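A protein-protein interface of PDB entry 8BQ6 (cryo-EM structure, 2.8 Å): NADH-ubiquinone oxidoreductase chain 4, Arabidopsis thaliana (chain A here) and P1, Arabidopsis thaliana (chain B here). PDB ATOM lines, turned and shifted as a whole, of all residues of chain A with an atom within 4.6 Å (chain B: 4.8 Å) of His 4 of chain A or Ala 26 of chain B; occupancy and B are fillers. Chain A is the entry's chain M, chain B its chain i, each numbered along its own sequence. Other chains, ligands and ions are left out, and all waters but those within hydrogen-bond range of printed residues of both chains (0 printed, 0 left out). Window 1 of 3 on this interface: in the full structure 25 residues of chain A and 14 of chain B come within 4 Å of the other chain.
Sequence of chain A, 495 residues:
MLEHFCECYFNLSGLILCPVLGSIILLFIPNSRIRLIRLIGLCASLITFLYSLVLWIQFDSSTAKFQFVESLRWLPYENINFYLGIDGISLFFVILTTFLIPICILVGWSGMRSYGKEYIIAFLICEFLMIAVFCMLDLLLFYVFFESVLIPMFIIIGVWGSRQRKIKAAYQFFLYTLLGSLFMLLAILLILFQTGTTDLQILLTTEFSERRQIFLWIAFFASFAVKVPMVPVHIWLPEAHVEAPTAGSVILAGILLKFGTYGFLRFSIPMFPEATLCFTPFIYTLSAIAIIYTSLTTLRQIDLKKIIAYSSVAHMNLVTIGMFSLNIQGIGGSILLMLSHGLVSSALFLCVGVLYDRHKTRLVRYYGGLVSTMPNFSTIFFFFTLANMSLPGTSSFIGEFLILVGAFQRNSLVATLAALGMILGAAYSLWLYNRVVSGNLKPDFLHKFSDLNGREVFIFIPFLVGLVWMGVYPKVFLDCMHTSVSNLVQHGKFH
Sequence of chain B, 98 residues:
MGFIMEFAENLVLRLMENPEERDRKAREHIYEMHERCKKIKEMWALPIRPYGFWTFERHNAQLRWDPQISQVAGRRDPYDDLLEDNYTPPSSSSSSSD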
ATOM      1  N   LEU A   2     -14.084  14.282  -5.558  1.00  0.00           N
ATOM      2  CA  LEU A   2     -14.516  14.870  -4.297  1.00  0.00           C
ATOM      3  C   LEU A   2     -15.727  14.131  -3.737  1.00  0.00           C
ATOM      4  O   LEU A   2     -16.802  14.151  -4.334  1.00  0.00           O
ATOM      5  CB  LEU A   2     -14.849  16.348  -4.484  1.00  0.00           C
ATOM      6  CG  LEU A   2     -14.929  17.137  -3.182  1.00  0.00           C
ATOM      7  CD1 LEU A   2     -13.540  17.251  -2.572  1.00  0.00           C
ATOM      8  CD2 LEU A   2     -15.536  18.501  -3.429  1.00  0.00           C
ATOM      9  N   GLU A   3     -15.492  13.362  -2.671  1.00  0.00           N
ATOM     10  CA  GLU A   3     -16.578  12.519  -2.112  1.00  0.00           C
ATOM     11  C   GLU A   3     -17.513  13.386  -1.275  1.00  0.00           C
ATOM     12  O   GLU A   3     -17.320  13.462  -0.044  1.00  0.00           O
ATOM     13  CB  GLU A   3     -15.989  11.342  -1.334  1.00  0.00           C
ATOM     14  CG  GLU A   3     -15.412  10.263  -2.236  1.00  0.00           C
ATOM     15  CD  GLU A   3     -16.142  10.025  -3.549  1.00  0.00           C
ATOM     16  OE1 GLU A   3     -17.267   9.486  -3.514  1.00  0.00           O
ATOM     17  OE2 GLU A   3     -15.573  10.363  -4.608  1.00  0.00           O
ATOM     18  N   HIS A   4     -18.489  14.007  -1.932  1.00  0.00           N
ATOM     19  CA  HIS A   4     -19.495  14.831  -1.222  1.00  0.00           C
ATOM     20  C   HIS A   4     -20.579  13.870  -0.728  1.00  0.00           C
ATOM     21  O   HIS A   4     -21.695  13.952  -1.245  1.00  0.00           O
ATOM     22  CB  HIS A   4     -19.955  15.950  -2.173  1.00  0.00           C
ATOM     23  CG  HIS A   4     -20.818  17.015  -1.574  1.00  0.00           C
ATOM     24  ND1 HIS A   4     -20.947  18.261  -2.158  1.00  0.00           N
ATOM     25  CD2 HIS A   4     -21.613  17.029  -0.482  1.00  0.00           C
ATOM     26  CE1 HIS A   4     -21.776  18.998  -1.445  1.00  0.00           C
ATOM     27  NE2 HIS A   4     -22.196  18.265  -0.410  1.00  0.00           N
ATOM     28  N   PHE A   5     -20.238  12.956   0.190  1.00  0.00           N
ATOM     29  CA  PHE A   5     -21.243  12.040   0.794  1.00  0.00           C
ATOM     30  C   PHE A   5     -22.036  12.794   1.865  1.00  0.00           C
ATOM     31  O   PHE A   5     -21.539  13.818   2.374  1.00  0.00           O
ATOM     32  CB  PHE A   5     -20.563  10.805   1.391  1.00  0.00           C
ATOM     33  CG  PHE A   5     -21.432   9.573   1.389  1.00  0.00           C
ATOM     34  CD1 PHE A   5     -22.199   9.251   0.280  1.00  0.00           C
ATOM     35  CD2 PHE A   5     -21.500   8.747   2.499  1.00  0.00           C
ATOM     36  CE1 PHE A   5     -23.007   8.126   0.278  1.00  0.00           C
ATOM     37  CE2 PHE A   5     -22.307   7.620   2.495  1.00  0.00           C
ATOM     38  CZ  PHE A   5     -23.059   7.311   1.385  1.00  0.00           C
ATOM     39  N   CYS A   6     -23.218  12.287   2.230  1.00  0.00           N
ATOM     40  CA  CYS A   6     -24.090  13.008   3.198  1.00  0.00           C
ATOM     41  C   CYS A   6     -23.931  12.449   4.619  1.00  0.00           C
ATOM     42  O   CYS A   6     -23.505  11.281   4.750  1.00  0.00           O
ATOM     43  CB  CYS A   6     -25.549  12.889   2.776  1.00  0.00           C
ATOM     44  SG  CYS A   6     -26.648  14.024   3.661  1.00  0.00           S
ATOM     45  N   LYS A  65     -29.166  25.780  -1.400  1.00  0.00           N
ATOM     46  CA  LYS A  65     -28.254  24.751  -1.864  1.00  0.00           C
ATOM     47  C   LYS A  65     -29.016  23.446  -2.074  1.00  0.00           C
ATOM     48  O   LYS A  65     -30.149  23.272  -1.621  1.00  0.00           O
ATOM     49  CB  LYS A  65     -27.110  24.564  -0.871  1.00  0.00           C
ATOM     50  CG  LYS A  65     -25.931  25.512  -1.062  1.00  0.00           C
ATOM     51  CD  LYS A  65     -26.216  26.895  -0.495  1.00  0.00           C
ATOM     52  CE  LYS A  65     -25.279  27.947  -1.072  1.00  0.00           C
ATOM     53  NZ  LYS A  65     -24.979  29.011  -0.074  1.00  0.00           N
ATOM     54  N   VAL A  69     -27.001  15.949  -0.526  1.00  0.00           N
ATOM     55  CA  VAL A  69     -26.110  15.681  -1.697  1.00  0.00           C
ATOM     56  C   VAL A  69     -25.193  14.504  -1.392  1.00  0.00           C
ATOM     57  O   VAL A  69     -24.503  14.542  -0.357  1.00  0.00           O
ATOM     58  CB  VAL A  69     -25.282  16.904  -2.136  1.00  0.00           C
ATOM     59  CG1 VAL A  69     -24.292  16.554  -3.237  1.00  0.00           C
ATOM     60  CG2 VAL A  69     -26.175  18.032  -2.602  1.00  0.00           C
ATOM     61  N   GLU A  70     -25.214  13.497  -2.258  1.00  0.00           N
ATOM     62  CA  GLU A  70     -24.277  12.362  -2.097  1.00  0.00           C
ATOM     63  C   GLU A  70     -23.612  12.135  -3.451  1.00  0.00           C
ATOM     64  O   GLU A  70     -24.274  12.333  -4.491  1.00  0.00           O
ATOM     65  CB  GLU A  70     -24.970  11.140  -1.499  1.00  0.00           C
ATOM     66  CG  GLU A  70     -25.587  10.204  -2.510  1.00  0.00           C
ATOM     67  CD  GLU A  70     -26.672   9.366  -1.870  1.00  0.00           C
ATOM     68  OE1 GLU A  70     -26.412   8.797  -0.800  1.00  0.00           O
ATOM     69  OE2 GLU A  70     -27.766   9.304  -2.434  1.00  0.00           O
ATOM     70  N   SER A  71     -22.327  11.801  -3.430  1.00  0.00           N
ATOM     71  CA  SER A  71     -21.584  11.652  -4.702  1.00  0.00           C
ATOM     72  C   SER A  71     -21.466  10.173  -5.054  1.00  0.00           C
ATOM     73  O   SER A  71     -21.370   9.349  -4.130  1.00  0.00           O
ATOM     74  CB  SER A  71     -20.234  12.296  -4.608  1.00  0.00           C
ATOM     75  OG  SER A  71     -19.429  11.641  -3.640  1.00  0.00           O
ATOM     76  N   TYR A  83     -23.448  13.337  -8.967  1.00  0.00           N
ATOM     77  CA  TYR A  83     -24.011  13.793  -7.707  1.00  0.00           C
ATOM     78  C   TYR A  83     -25.524  13.641  -7.722  1.00  0.00           C
ATOM     79  O   TYR A  83     -26.165  13.795  -8.767  1.00  0.00           O
ATOM     80  CB  TYR A  83     -23.637  15.255  -7.435  1.00  0.00           C
ATOM     81  CG  TYR A  83     -22.151  15.493  -7.320  1.00  0.00           C
ATOM     82  CD1 TYR A  83     -21.335  15.466  -8.443  1.00  0.00           C
ATOM     83  CD2 TYR A  83     -21.560  15.735  -6.088  1.00  0.00           C
ATOM     84  CE1 TYR A  83     -19.981  15.673  -8.346  1.00  0.00           C
ATOM     85  CE2 TYR A  83     -20.202  15.945  -5.981  1.00  0.00           C
ATOM     86  CZ  TYR A  83     -19.417  15.913  -7.113  1.00  0.00           C
ATOM     87  OH  TYR A  83     -18.063  16.124  -7.019  1.00  0.00           O
ATOM     88  N   ARG B  22     -22.677  21.395   5.126  1.00  0.00           N
ATOM     89  CA  ARG B  22     -23.344  21.234   3.840  1.00  0.00           C
ATOM     90  C   ARG B  22     -23.004  22.386   2.901  1.00  0.00           C
ATOM     91  O   ARG B  22     -22.772  22.179   1.706  1.00  0.00           O
ATOM     92  CB  ARG B  22     -24.852  21.123   4.056  1.00  0.00           C
ATOM     93  CG  ARG B  22     -25.638  20.825   2.802  1.00  0.00           C
ATOM     94  CD  ARG B  22     -26.618  21.938   2.487  1.00  0.00           C
ATOM     95  NE  ARG B  22     -27.714  21.997   3.446  1.00  0.00           N
ATOM     96  CZ  ARG B  22     -28.013  23.061   4.178  1.00  0.00           C
ATOM     97  NH1 ARG B  22     -27.324  24.185   4.078  1.00  0.00           N
ATOM     98  NH2 ARG B  22     -29.035  22.999   5.025  1.00  0.00           N
ATOM     99  N   ASP B  23     -22.975  23.615   3.426  1.00  0.00           N
ATOM    100  CA  ASP B  23     -22.572  24.747   2.595  1.00  0.00           C
ATOM    101  C   ASP B  23     -21.080  24.716   2.285  1.00  0.00           C
ATOM    102  O   ASP B  23     -20.668  25.082   1.175  1.00  0.00           O
ATOM    103  CB  ASP B  23     -22.937  26.066   3.275  1.00  0.00           C
ATOM    104  CG  ASP B  23     -24.418  26.173   3.600  1.00  0.00           C
ATOM    105  OD1 ASP B  23     -25.256  25.725   2.789  1.00  0.00           O
ATOM    106  OD2 ASP B  23     -24.743  26.712   4.675  1.00  0.00           O
ATOM    107  N   ARG B  24     -20.259  24.293   3.248  1.00  0.00           N
ATOM    108  CA  ARG B  24     -18.820  24.202   3.032  1.00  0.00           C
ATOM    109  C   ARG B  24     -18.496  23.280   1.862  1.00  0.00           C
ATOM    110  O   ARG B  24     -17.782  23.673   0.930  1.00  0.00           O
ATOM    111  CB  ARG B  24     -18.144  23.719   4.317  1.00  0.00           C
ATOM    112  CG  ARG B  24     -16.735  24.240   4.543  1.00  0.00           C
ATOM    113  CD  ARG B  24     -16.132  23.598   5.786  1.00  0.00           C
ATOM    114  NE  ARG B  24     -16.203  22.141   5.757  1.00  0.00           N
ATOM    115  CZ  ARG B  24     -15.609  21.364   4.860  1.00  0.00           C
ATOM    116  NH1 ARG B  24     -14.789  21.858   3.949  1.00  0.00           N
ATOM    117  NH2 ARG B  24     -15.825  20.052   4.895  1.00  0.00           N
ATOM    118  N   LYS B  25     -19.047  22.068   1.900  1.00  0.00           N
ATOM    119  CA  LYS B  25     -18.781  21.074   0.828  1.00  0.00           C
ATOM    120  C   LYS B  25     -19.304  21.592  -0.517  1.00  0.00           C
ATOM    121  O   LYS B  25     -18.642  21.329  -1.528  1.00  0.00           O
ATOM    122  CB  LYS B  25     -19.393  19.727   1.218  1.00  0.00           C
ATOM    123  CG  LYS B  25     -18.625  18.935   2.265  1.00  0.00           C
ATOM    124  CD  LYS B  25     -19.338  17.672   2.694  1.00  0.00           C
ATOM    125  CE  LYS B  25     -20.754  17.919   3.169  1.00  0.00           C
ATOM    126  NZ  LYS B  25     -21.567  16.680   3.145  1.00  0.00           N
ATOM    127  N   ALA B  26     -20.439  22.295  -0.533  1.00  0.00           N
ATOM    128  CA  ALA B  26     -20.952  22.875  -1.769  1.00  0.00           C
ATOM    129  C   ALA B  26     -19.977  23.897  -2.338  1.00  0.00           C
ATOM    130  O   ALA B  26     -19.734  23.928  -3.550  1.00  0.00           O
ATOM    131  CB  ALA B  26     -22.318  23.511  -1.521  1.00  0.00           C
ATOM    132  N   ARG B  27     -19.406  24.741  -1.475  1.00  0.00           N
ATOM    133  CA  ARG B  27     -18.416  25.709  -1.942  1.00  0.00           C
ATOM    134  C   ARG B  27     -17.178  25.022  -2.509  1.00  0.00           C
ATOM    135  O   ARG B  27     -16.672  25.415  -3.572  1.00  0.00           O
ATOM    136  CB  ARG B  27     -18.020  26.645  -0.806  1.00  0.00           C
ATOM    137  CG  ARG B  27     -19.042  27.704  -0.482  1.00  0.00           C
ATOM    138  CD  ARG B  27     -18.408  28.774   0.371  1.00  0.00           C
ATOM    139  NE  ARG B  27     -17.708  28.198   1.513  1.00  0.00           N
ATOM    140  CZ  ARG B  27     -18.276  27.932   2.681  1.00  0.00           C
ATOM    141  NH1 ARG B  27     -19.559  28.166   2.895  1.00  0.00           N
ATOM    142  NH2 ARG B  27     -17.533  27.423   3.661  1.00  0.00           N
ATOM    143  N   GLU B  28     -16.665  24.010  -1.804  1.00  0.00           N
ATOM    144  CA  GLU B  28     -15.455  23.345  -2.281  1.00  0.00           C
ATOM    145  C   GLU B  28     -15.691  22.664  -3.617  1.00  0.00           C
ATOM    146  O   GLU B  28     -14.813  22.668  -4.485  1.00  0.00           O
ATOM    147  CB  GLU B  28     -14.936  22.330  -1.266  1.00  0.00           C
ATOM    148  CG  GLU B  28     -13.887  22.881  -0.336  1.00  0.00           C
ATOM    149  CD  GLU B  28     -14.037  22.352   1.065  1.00  0.00           C
ATOM    150  OE1 GLU B  28     -14.117  21.115   1.233  1.00  0.00           O
ATOM    151  OE2 GLU B  28     -14.084  23.173   2.000  1.00  0.00           O
ATOM    152  N   HIS B  29     -16.865  22.062  -3.798  1.00  0.00           N
ATOM    153  CA  HIS B  29     -17.161  21.393  -5.059  1.00  0.00           C
ATOM    154  C   HIS B  29     -16.979  22.354  -6.232  1.00  0.00           C
ATOM    155  O   HIS B  29     -16.263  22.052  -7.200  1.00  0.00           O
ATOM    156  CB  HIS B  29     -18.579  20.819  -5.003  1.00  0.00           C
ATOM    157  CG  HIS B  29     -19.122  20.392  -6.328  1.00  0.00           C
ATOM    158  ND1 HIS B  29     -18.946  19.120  -6.830  1.00  0.00           N
ATOM    159  CD2 HIS B  29     -19.871  21.055  -7.242  1.00  0.00           C
ATOM    160  CE1 HIS B  29     -19.542  19.025  -8.004  1.00  0.00           C
ATOM    161  NE2 HIS B  29     -20.113  20.185  -8.276  1.00  0.00           N
ATOM    162  N   ILE B  30     -17.554  23.553  -6.116  1.00  0.00           N
ATOM    163  CA  ILE B  30     -17.458  24.550  -7.179  1.00  0.00           C
ATOM    164  C   ILE B  30     -16.017  25.017  -7.361  1.00  0.00           C
ATOM    165  O   ILE B  30     -15.515  25.109  -8.491  1.00  0.00           O
ATOM    166  CB  ILE B  30     -18.395  25.732  -6.877  1.00  0.00           C
ATOM    167  CG1 ILE B  30     -19.800  25.220  -6.561  1.00  0.00           C
ATOM    168  CG2 ILE B  30     -18.418  26.698  -8.040  1.00  0.00           C
ATOM    169  CD1 ILE B  30     -20.896  26.215  -6.854  1.00  0.00           C
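His 4 of chain A touches just these residues of chain B: Lys 25 and Ala 26.
Of chain A, only His 4 (3.7 Å) comes within 4 Å of Ala 26 of chain B.
Of the printed residues of chain A, Lys 25 of chain B touches His 4 and Phe 5.
Of the printed residues of chain A, His 29 of chain B touches Leu 2 (3.7 Å) and Tyr 83 (3.1 Å).
Of the printed residues of chain B, Tyr 83 of chain A touches His 29.
Of the printed residues of chain B, Phe 5 of chain A touches Lys 25 (3.0 Å).
Printed residues of chain A within 4 Å of Asp 23 of chain B: Lys 65.
The nearest printed residue of chain A that does not touch Asp 23 of chain B is His 4 of chain A (6.6 Å).
The backbone NH of His 4 of chain A sits at hydrogen-bond distance from the side-chain hydroxyl of Ser 71 of chain A (3.1 Å).
The side-chain carboxylate of Asp 23 of chain B lies within salt-bridge range of the guanidinium group of Arg 22 of chain B, at 2.9 Å.
The backbone carbonyl oxygen (O) of Phe 5 of chain A sits at hydrogen-bond distance from the side-chain amino group (NZ) of Lys 25 of chain B, 3.0 Å away.
OH of Tyr 83 of chain A sits at hydrogen-bond distance from ND1 of His 29 of chain B, at 3.1 Å.
Of the 9 printed residues of chain B, 4 touch a printed residue of chain A.
Along chain B the printed residues that touch a printed residue of chain A span positions 23 to 29.
Hydrophobic or aromatic side chains of chain A that line the printed part of chain B: Leu 2, His 4 and Tyr 83.
Leu 2 of chain A touches His 29 of chain B.
His 4 of chain A touches Lys 25 of chain B.
Ala 26 of chain B touches His 4 of chain A (N to CE1, 3.7 Å).
CD of Lys 65 of chain A touches OD1 of Asp 23 of chain B, 3.6 Å away.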
